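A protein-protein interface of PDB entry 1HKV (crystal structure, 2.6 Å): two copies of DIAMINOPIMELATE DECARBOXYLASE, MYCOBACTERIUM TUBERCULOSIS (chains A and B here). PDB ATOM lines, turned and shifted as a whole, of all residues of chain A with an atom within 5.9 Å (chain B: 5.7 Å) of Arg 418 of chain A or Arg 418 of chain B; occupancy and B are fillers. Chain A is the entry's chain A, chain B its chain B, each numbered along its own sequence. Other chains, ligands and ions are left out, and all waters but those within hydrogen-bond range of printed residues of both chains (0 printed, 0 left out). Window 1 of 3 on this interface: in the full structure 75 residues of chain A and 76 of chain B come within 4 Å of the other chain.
Among the printed residues, merely in contact across the chains: Ser 410 of chain A with Ser 411 of chain B (3.3 Å), Ser 411 of chain A with Ser 410 of chain B (3.3 Å), Leu 444 of chain A with Tyr 407 of chain B (3.3 Å), Tyr 407 of chain A with Leu 444 of chain B (3.4 Å), Glu 436 of chain A with Leu 444 of chain B (3.8 Å), Leu 444 of chain A with Glu 436 of chain B (3.8 Å) and Arg 412 of chain A with Arg 412 of chain B (3.8 Å).
Ser 410 of chain A touches Ser 411 of chain B, and with the chains exchanged Ser 411 of chain A touches Ser 410 of chain B. Arg 412 of chain A touches Arg 418 of chain B, and with the chains exchanged Arg 418 of chain A touches Arg 412 of chain B. Arg 418 of chain A touches its own counterpart, Arg 418 of chain B. Arg 434 of chain A touches Leu 444 of chain B, and with the chains exchanged Leu 444 of chain A touches Arg 434 of chain B. Positions printed for both chains: 407, 410, 411, 412, 416, 417, 418, 419, 420, 434, 435, 436 and 444.
Hydrophobic or aromatic side chains of chain B within 4 Å of the printed part of chain A: Tyr 407 and Leu 444. Of the 13 printed residues of chain A, 8 touch a printed residue of chain B. Printed residues of chain A that touch a printed residue of chain B: Tyr 407, Ser 410, Ser 411, Arg 412, Arg 418, Arg 434, Glu 436 and Leu 444. Hydrophobic or aromatic side chains of chain A within 4 Å of the printed part of chain B: Tyr 407 and Leu 444. Among the printed residues, 12 pairs touch across the chains.
The guanidinium group of Arg 418 of chain A sits at hydrogen-bond distance from the backbone carbonyl oxygen of Ser 410 of chain A, 2.9 Å away. The guanidinium group (NE) of Arg 412 of chain A is in salt-bridge range of the side-chain carboxylate (OE1) of Glu 436 of chain A. NE of Arg 418 of chain A is in salt-bridge range of OE2 of Glu 436 of chain A (3.6 Å). The side-chain hydroxyl (OG) of Ser 410 of chain B is in hydrogen-bond range of the backbone carbonyl oxygen (O) of Tyr 407 of chain B (2.8 Å). NH1 of Arg 418 of chain B sits at hydrogen-bond distance from O of Ser 410 of chain B. The guanidinium group (NH2) of Arg 412 of chain B lies within salt-bridge range of the side-chain carboxylate (OE2) of Glu 436 of chain B (2.8 Å).
The backbone NH of Arg 434 of chain A lies within hydrogen-bond range of the backbone carbonyl oxygen of Leu 444 of chain B (3.1 Å). N of Arg 434 of chain B lies within hydrogen-bond range of O of Leu 444 of chain A (3.1 Å). The guanidinium group (NH2) of Arg 418 of chain B lies close to the guanidinium group (NE) of Arg 412 of chain A (3.2 Å). NH1 of Arg 418 of chain A lies close to NE of Arg 412 of chain B, 3.1 Å away. The guanidinium group (NH1) of Arg 418 of chain A lies close to the guanidinium group (NH2) of Arg 418 of chain B.
Arg 418 of chain A touches two residues of chain B. Printed residues of chain B within 4 Å of Arg 434 of chain A: Leu 444. Of the printed residues of chain B, Leu 444 of chain A touches Tyr 407 (3.3 Å), Arg 434 (3.1 Å) and Glu 436 (3.8 Å). Printed residues of chain A within 4 Å of Ser 410 of chain B: Ser 411 (3.3 Å). Arg 418 of chain B touches two residues of chain A. Of the printed residues of chain A, Leu 444 of chain B touches Tyr 407 (3.4 Å), Arg 434 (3.1 Å) and Glu 436 (3.8 Å). The nearest residue of chain B that does not touch Arg 418 of chain A is Leu 444 of chain B (4.4 Å). The nearest residue of chain A that does not touch Arg 418 of chain B is Leu 444 of chain A (4.2 Å).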
ATOM      1  N   TYR A 407      -6.535   1.351 -18.377  1.00  0.00           N
ATOM      2  CA  TYR A 407      -5.431   1.088 -17.488  1.00  0.00           C
ATOM      3  C   TYR A 407      -4.666  -0.213 -17.877  1.00  0.00           C
ATOM      4  O   TYR A 407      -3.392  -0.225 -17.857  1.00  0.00           O
ATOM      5  CB  TYR A 407      -5.939   1.012 -16.031  1.00  0.00           C
ATOM      6  CG  TYR A 407      -4.843   0.957 -15.008  1.00  0.00           C
ATOM      7  CD1 TYR A 407      -4.214  -0.231 -14.680  1.00  0.00           C
ATOM      8  CD2 TYR A 407      -4.441   2.067 -14.368  1.00  0.00           C
ATOM      9  CE1 TYR A 407      -3.146  -0.263 -13.724  1.00  0.00           C
ATOM     10  CE2 TYR A 407      -3.437   2.040 -13.441  1.00  0.00           C
ATOM     11  CZ  TYR A 407      -2.788   0.871 -13.127  1.00  0.00           C
ATOM     12  OH  TYR A 407      -1.765   0.901 -12.205  1.00  0.00           O
ATOM     13  N   SER A 410      -2.247   0.493 -20.375  1.00  0.00           N
ATOM     14  CA  SER A 410      -1.405   1.653 -20.036  1.00  0.00           C
ATOM     15  C   SER A 410       0.028   1.322 -20.214  1.00  0.00           C
ATOM     16  O   SER A 410       0.421   0.225 -19.944  1.00  0.00           O
ATOM     17  CB  SER A 410      -1.599   2.043 -18.585  1.00  0.00           C
ATOM     18  OG  SER A 410      -1.282   0.978 -17.710  1.00  0.00           O
ATOM     19  N   SER A 411       0.816   2.301 -20.655  1.00  0.00           N
ATOM     20  CA  SER A 411       2.219   2.125 -20.881  1.00  0.00           C
ATOM     21  C   SER A 411       3.041   3.253 -20.200  1.00  0.00           C
ATOM     22  O   SER A 411       2.487   4.045 -19.444  1.00  0.00           O
ATOM     23  CB  SER A 411       2.490   2.059 -22.384  1.00  0.00           C
ATOM     24  OG  SER A 411       2.262   3.273 -23.048  1.00  0.00           O
ATOM     25  N   ARG A 412       4.367   3.255 -20.411  1.00  0.00           N
ATOM     26  CA  ARG A 412       5.229   4.321 -19.928  1.00  0.00           C
ATOM     27  C   ARG A 412       5.851   5.012 -21.134  1.00  0.00           C
ATOM     28  O   ARG A 412       7.034   5.321 -21.161  1.00  0.00           O
ATOM     29  CB  ARG A 412       6.351   3.796 -19.015  1.00  0.00           C
ATOM     30  CG  ARG A 412       5.910   3.103 -17.772  1.00  0.00           C
ATOM     31  CD  ARG A 412       7.053   2.432 -17.047  1.00  0.00           C
ATOM     32  NE  ARG A 412       6.677   1.864 -15.725  1.00  0.00           N
ATOM     33  CZ  ARG A 412       7.453   1.020 -15.054  1.00  0.00           C
ATOM     34  NH1 ARG A 412       8.637   0.647 -15.576  1.00  0.00           N
ATOM     35  NH2 ARG A 412       7.049   0.533 -13.874  1.00  0.00           N
ATOM     36  N   VAL A 416       6.102   8.238 -18.989  1.00  0.00           N
ATOM     37  CA  VAL A 416       4.985   8.766 -18.254  1.00  0.00           C
ATOM     38  C   VAL A 416       4.394   7.669 -17.371  1.00  0.00           C
ATOM     39  O   VAL A 416       3.840   6.709 -17.866  1.00  0.00           O
ATOM     40  CB  VAL A 416       3.924   9.321 -19.212  1.00  0.00           C
ATOM     41  CG1 VAL A 416       2.695   9.821 -18.475  1.00  0.00           C
ATOM     42  CG2 VAL A 416       4.513  10.434 -20.067  1.00  0.00           C
ATOM     43  N   GLY A 417       4.495   7.806 -16.069  1.00  0.00           N
ATOM     44  CA  GLY A 417       4.072   6.721 -15.175  1.00  0.00           C
ATOM     45  C   GLY A 417       2.574   6.505 -15.175  1.00  0.00           C
ATOM     46  O   GLY A 417       1.861   7.315 -15.695  1.00  0.00           O
ATOM     47  N   ARG A 418       2.108   5.423 -14.589  1.00  0.00           N
ATOM     48  CA  ARG A 418       0.733   5.133 -14.642  1.00  0.00           C
ATOM     49  C   ARG A 418       0.033   6.077 -13.726  1.00  0.00           C
ATOM     50  O   ARG A 418       0.529   6.404 -12.727  1.00  0.00           O
ATOM     51  CB  ARG A 418       0.453   3.655 -14.236  1.00  0.00           C
ATOM     52  CG  ARG A 418       1.217   2.628 -14.994  1.00  0.00           C
ATOM     53  CD  ARG A 418       0.533   1.199 -15.119  1.00  0.00           C
ATOM     54  NE  ARG A 418       1.583   0.176 -15.261  1.00  0.00           N
ATOM     55  CZ  ARG A 418       2.325  -0.063 -16.394  1.00  0.00           C
ATOM     56  NH1 ARG A 418       3.281  -0.946 -16.350  1.00  0.00           N
ATOM     57  NH2 ARG A 418       2.096   0.553 -17.548  1.00  0.00           N
ATOM     58  N   PRO A 419      -1.145   6.513 -14.050  1.00  0.00           N
ATOM     59  CA  PRO A 419      -1.915   7.278 -13.100  1.00  0.00           C
ATOM     60  C   PRO A 419      -2.367   6.453 -11.918  1.00  0.00           C
ATOM     61  O   PRO A 419      -2.423   5.234 -11.968  1.00  0.00           O
ATOM     62  CB  PRO A 419      -3.090   7.718 -13.909  1.00  0.00           C
ATOM     63  CG  PRO A 419      -2.630   7.661 -15.186  1.00  0.00           C
ATOM     64  CD  PRO A 419      -1.856   6.393 -15.306  1.00  0.00           C
ATOM     65  N   ALA A 420      -2.679   7.145 -10.840  1.00  0.00           N
ATOM     66  CA  ALA A 420      -3.229   6.520  -9.651  1.00  0.00           C
ATOM     67  C   ALA A 420      -4.646   6.158  -9.931  1.00  0.00           C
ATOM     68  O   ALA A 420      -5.264   6.714 -10.812  1.00  0.00           O
ATOM     69  CB  ALA A 420      -3.150   7.490  -8.451  1.00  0.00           C
ATOM     70  N   ARG A 434      -1.686   3.052  -6.375  1.00  0.00           N
ATOM     71  CA  ARG A 434      -0.960   4.281  -6.360  1.00  0.00           C
ATOM     72  C   ARG A 434      -0.300   4.610  -7.687  1.00  0.00           C
ATOM     73  O   ARG A 434      -0.197   3.808  -8.511  1.00  0.00           O
ATOM     74  CB  ARG A 434       0.071   4.283  -5.238  1.00  0.00           C
ATOM     75  CG  ARG A 434       0.972   3.201  -5.317  1.00  0.00           C
ATOM     76  CD  ARG A 434       2.338   3.649  -5.201  1.00  0.00           C
ATOM     77  NE  ARG A 434       3.288   2.540  -5.162  1.00  0.00           N
ATOM     78  CZ  ARG A 434       4.459   2.585  -5.827  1.00  0.00           C
ATOM     79  NH1 ARG A 434       4.782   3.646  -6.585  1.00  0.00           N
ATOM     80  NH2 ARG A 434       5.287   1.550  -5.821  1.00  0.00           N
ATOM     81  N   ARG A 435       0.099   5.860  -7.813  1.00  0.00           N
ATOM     82  CA  ARG A 435       0.652   6.408  -9.000  1.00  0.00           C
ATOM     83  C   ARG A 435       2.154   6.066  -9.084  1.00  0.00           C
ATOM     84  O   ARG A 435       2.858   6.093  -8.071  1.00  0.00           O
ATOM     85  CB  ARG A 435       0.448   7.933  -8.945  1.00  0.00           C
ATOM     86  CG  ARG A 435       1.521   8.810  -9.634  1.00  0.00           C
ATOM     87  CD  ARG A 435       1.178  10.371  -9.664  1.00  0.00           C
ATOM     88  NE  ARG A 435      -0.094  10.661 -10.344  1.00  0.00           N
ATOM     89  CZ  ARG A 435      -1.256  10.814  -9.720  1.00  0.00           C
ATOM     90  NH1 ARG A 435      -2.365  11.043 -10.383  1.00  0.00           N
ATOM     91  NH2 ARG A 435      -1.305  10.714  -8.431  1.00  0.00           N
ATOM     92  N   GLU A 436       2.641   5.754 -10.274  1.00  0.00           N
ATOM     93  CA  GLU A 436       4.043   5.418 -10.450  1.00  0.00           C
ATOM     94  C   GLU A 436       4.877   6.632 -10.271  1.00  0.00           C
ATOM     95  O   GLU A 436       4.425   7.705 -10.419  1.00  0.00           O
ATOM     96  CB  GLU A 436       4.350   4.792 -11.846  1.00  0.00           C
ATOM     97  CG  GLU A 436       3.707   3.403 -12.102  1.00  0.00           C
ATOM     98  CD  GLU A 436       4.289   2.652 -13.302  1.00  0.00           C
ATOM     99  OE1 GLU A 436       4.660   3.302 -14.299  1.00  0.00           O
ATOM    100  OE2 GLU A 436       4.367   1.382 -13.242  1.00  0.00           O
ATOM    101  N   LEU A 444      13.573  -1.404 -13.093  1.00  0.00           N
ATOM    102  CA  LEU A 444      14.094  -2.526 -13.890  1.00  0.00           C
ATOM    103  C   LEU A 444      15.548  -2.360 -14.257  1.00  0.00           C
ATOM    104  O   LEU A 444      16.213  -3.298 -14.644  1.00  0.00           O
ATOM    105  CB  LEU A 444      13.281  -2.692 -15.155  1.00  0.00           C
ATOM    106  CG  LEU A 444      11.799  -2.836 -14.917  1.00  0.00           C
ATOM    107  CD1 LEU A 444      11.149  -2.974 -16.271  1.00  0.00           C
ATOM    108  CD2 LEU A 444      11.453  -4.064 -13.984  1.00  0.00           C
ATOM    109  N   TYR B 407       9.695  -1.306 -27.004  1.00  0.00           N
ATOM    110  CA  TYR B 407       9.777  -1.411 -25.560  1.00  0.00           C
ATOM    111  C   TYR B 407       9.212  -0.122 -24.920  1.00  0.00           C
ATOM    112  O   TYR B 407       8.573  -0.198 -23.879  1.00  0.00           O
ATOM    113  CB  TYR B 407      11.236  -1.721 -25.111  1.00  0.00           C
ATOM    114  CG  TYR B 407      11.399  -1.876 -23.588  1.00  0.00           C
ATOM    115  CD1 TYR B 407      11.452  -0.755 -22.759  1.00  0.00           C
ATOM    116  CD2 TYR B 407      11.512  -3.132 -22.990  1.00  0.00           C
ATOM    117  CE1 TYR B 407      11.562  -0.877 -21.374  1.00  0.00           C
ATOM    118  CE2 TYR B 407      11.636  -3.250 -21.606  1.00  0.00           C
ATOM    119  CZ  TYR B 407      11.669  -2.097 -20.810  1.00  0.00           C
ATOM    120  OH  TYR B 407      11.815  -2.180 -19.446  1.00  0.00           O
ATOM    121  N   SER B 410       5.698  -0.482 -24.487  1.00  0.00           N
ATOM    122  CA  SER B 410       5.357  -1.757 -23.841  1.00  0.00           C
ATOM    123  C   SER B 410       4.411  -1.524 -22.761  1.00  0.00           C
ATOM    124  O   SER B 410       4.534  -0.564 -22.092  1.00  0.00           O
ATOM    125  CB  SER B 410       6.578  -2.444 -23.289  1.00  0.00           C
ATOM    126  OG  SER B 410       7.042  -1.798 -22.156  1.00  0.00           O
ATOM    127  N   SER B 411       3.452  -2.429 -22.608  1.00  0.00           N
ATOM    128  CA  SER B 411       2.449  -2.387 -21.523  1.00  0.00           C
ATOM    129  C   SER B 411       2.403  -3.721 -20.767  1.00  0.00           C
ATOM    130  O   SER B 411       3.117  -4.604 -21.116  1.00  0.00           O
ATOM    131  CB  SER B 411       1.096  -2.153 -22.125  1.00  0.00           C
ATOM    132  OG  SER B 411       0.590  -3.343 -22.777  1.00  0.00           O
ATOM    133  N   ARG B 412       1.510  -3.866 -19.788  1.00  0.00           N
ATOM    134  CA  ARG B 412       1.281  -5.161 -19.105  1.00  0.00           C
ATOM    135  C   ARG B 412      -0.060  -5.711 -19.427  1.00  0.00           C
ATOM    136  O   ARG B 412      -0.802  -6.073 -18.548  1.00  0.00           O
ATOM    137  CB  ARG B 412       1.336  -4.984 -17.554  1.00  0.00           C
ATOM    138  CG  ARG B 412       2.630  -4.339 -17.038  1.00  0.00           C
ATOM    139  CD  ARG B 412       2.542  -3.935 -15.538  1.00  0.00           C
ATOM    140  NE  ARG B 412       3.897  -3.691 -15.014  1.00  0.00           N
ATOM    141  CZ  ARG B 412       4.141  -3.064 -13.933  1.00  0.00           C
ATOM    142  NH1 ARG B 412       3.149  -2.572 -13.196  1.00  0.00           N
ATOM    143  NH2 ARG B 412       5.380  -2.901 -13.577  1.00  0.00           N
ATOM    144  N   VAL B 416       1.112  -9.444 -18.658  1.00  0.00           N
ATOM    145  CA  VAL B 416       2.324 -10.006 -19.237  1.00  0.00           C
ATOM    146  C   VAL B 416       3.397  -9.011 -19.056  1.00  0.00           C
ATOM    147  O   VAL B 416       3.343  -7.909 -19.646  1.00  0.00           O
ATOM    148  CB  VAL B 416       2.213 -10.271 -20.742  1.00  0.00           C
ATOM    149  CG1 VAL B 416       3.563 -10.787 -21.331  1.00  0.00           C
ATOM    150  CG2 VAL B 416       1.164 -11.216 -21.011  1.00  0.00           C
ATOM    151  N   GLY B 417       4.408  -9.375 -18.272  1.00  0.00           N
ATOM    152  CA  GLY B 417       5.404  -8.418 -17.863  1.00  0.00           C
ATOM    153  C   GLY B 417       6.340  -8.070 -18.971  1.00  0.00           C
ATOM    154  O   GLY B 417       6.444  -8.814 -19.966  1.00  0.00           O
ATOM    155  N   ARG B 418       7.038  -6.943 -18.791  1.00  0.00           N
ATOM    156  CA  ARG B 418       7.982  -6.465 -19.759  1.00  0.00           C
ATOM    157  C   ARG B 418       9.104  -7.482 -19.919  1.00  0.00           C
ATOM    158  O   ARG B 418       9.708  -7.910 -18.970  1.00  0.00           O
ATOM    159  CB  ARG B 418       8.545  -5.074 -19.365  1.00  0.00           C
ATOM    160  CG  ARG B 418       7.667  -3.928 -19.868  1.00  0.00           C
ATOM    161  CD  ARG B 418       8.147  -2.482 -19.539  1.00  0.00           C
ATOM    162  NE  ARG B 418       7.556  -1.987 -18.293  1.00  0.00           N
ATOM    163  CZ  ARG B 418       6.357  -1.344 -18.157  1.00  0.00           C
ATOM    164  NH1 ARG B 418       5.562  -1.060 -19.218  1.00  0.00           N
ATOM    165  NH2 ARG B 418       5.980  -0.974 -16.922  1.00  0.00           N
ATOM    166  N   PRO B 419       9.377  -7.858 -21.138  1.00  0.00           N
ATOM    167  CA  PRO B 419      10.547  -8.678 -21.438  1.00  0.00           C
ATOM    168  C   PRO B 419      11.880  -8.118 -20.859  1.00  0.00           C
ATOM    169  O   PRO B 419      11.970  -6.956 -20.467  1.00  0.00           O
ATOM    170  CB  PRO B 419      10.604  -8.638 -22.978  1.00  0.00           C
ATOM    171  CG  PRO B 419       9.249  -8.290 -23.400  1.00  0.00           C
ATOM    172  CD  PRO B 419       8.623  -7.492 -22.347  1.00  0.00           C
ATOM    173  N   ALA B 420      12.910  -8.954 -20.866  1.00  0.00           N
ATOM    174  CA  ALA B 420      14.265  -8.514 -20.532  1.00  0.00           C
ATOM    175  C   ALA B 420      14.904  -7.879 -21.694  1.00  0.00           C
ATOM    176  O   ALA B 420      14.663  -8.290 -22.820  1.00  0.00           O
ATOM    177  CB  ALA B 420      15.120  -9.704 -20.097  1.00  0.00           C
ATOM    178  N   ARG B 434      15.990  -5.726 -16.613  1.00  0.00           N
ATOM    179  CA  ARG B 434      15.547  -7.007 -16.153  1.00  0.00           C
ATOM    180  C   ARG B 434      14.114  -7.170 -16.486  1.00  0.00           C
ATOM    181  O   ARG B 434      13.436  -6.221 -16.785  1.00  0.00           O
ATOM    182  CB  ARG B 434      15.800  -7.126 -14.625  1.00  0.00           C
ATOM    183  CG  ARG B 434      14.604  -6.959 -13.662  1.00  0.00           C
ATOM    184  CD  ARG B 434      15.072  -6.810 -12.183  1.00  0.00           C
ATOM    185  NE  ARG B 434      14.337  -5.762 -11.464  1.00  0.00           N
ATOM    186  CZ  ARG B 434      13.014  -5.850 -11.162  1.00  0.00           C
ATOM    187  NH1 ARG B 434      12.291  -6.922 -11.551  1.00  0.00           N
ATOM    188  NH2 ARG B 434      12.400  -4.839 -10.508  1.00  0.00           N
ATOM    189  N   ARG B 435      13.650  -8.396 -16.395  1.00  0.00           N
ATOM    190  CA  ARG B 435      12.305  -8.782 -16.801  1.00  0.00           C
ATOM    191  C   ARG B 435      11.406  -8.622 -15.620  1.00  0.00           C
ATOM    192  O   ARG B 435      11.852  -8.742 -14.540  1.00  0.00           O
ATOM    193  CB  ARG B 435      12.361 -10.237 -17.312  1.00  0.00           C
ATOM    194  CG  ARG B 435      11.211 -11.173 -16.943  1.00  0.00           C
ATOM    195  CD  ARG B 435      11.367 -12.630 -17.550  1.00  0.00           C
ATOM    196  NE  ARG B 435      11.373 -12.670 -19.046  1.00  0.00           N
ATOM    197  CZ  ARG B 435      12.451 -12.644 -19.753  1.00  0.00           C
ATOM    198  NH1 ARG B 435      12.426 -12.695 -21.058  1.00  0.00           N
ATOM    199  NH2 ARG B 435      13.593 -12.579 -19.143  1.00  0.00           N
ATOM    200  N   GLU B 436      10.139  -8.282 -15.830  1.00  0.00           N
ATOM    201  CA  GLU B 436       9.245  -7.966 -14.714  1.00  0.00           C
ATOM    202  C   GLU B 436       8.723  -9.259 -14.186  1.00  0.00           C
ATOM    203  O   GLU B 436       8.831 -10.260 -14.839  1.00  0.00           O
ATOM    204  CB  GLU B 436       8.052  -7.052 -15.123  1.00  0.00           C
ATOM    205  CG  GLU B 436       8.445  -5.659 -15.665  1.00  0.00           C
ATOM    206  CD  GLU B 436       7.257  -4.649 -15.843  1.00  0.00           C
ATOM    207  OE1 GLU B 436       6.193  -4.966 -16.420  1.00  0.00           O
ATOM    208  OE2 GLU B 436       7.416  -3.540 -15.395  1.00  0.00           O
ATOM    209  N   LEU B 444       2.073  -1.789  -7.193  1.00  0.00           N
ATOM    210  CA  LEU B 444       1.400  -0.534  -7.064  1.00  0.00           C
ATOM    211  C   LEU B 444       0.180  -0.723  -6.220  1.00  0.00           C
ATOM    212  O   LEU B 444      -0.503   0.220  -5.908  1.00  0.00           O
ATOM    213  CB  LEU B 444       0.970  -0.004  -8.451  1.00  0.00           C
ATOM    214  CG  LEU B 444       2.019   0.187  -9.544  1.00  0.00           C
ATOM    215  CD1 LEU B 444       1.342   0.742 -10.802  1.00  0.00           C
ATOM    216  CD2 LEU B 444       3.170   1.106  -9.130  1.00  0.00           C
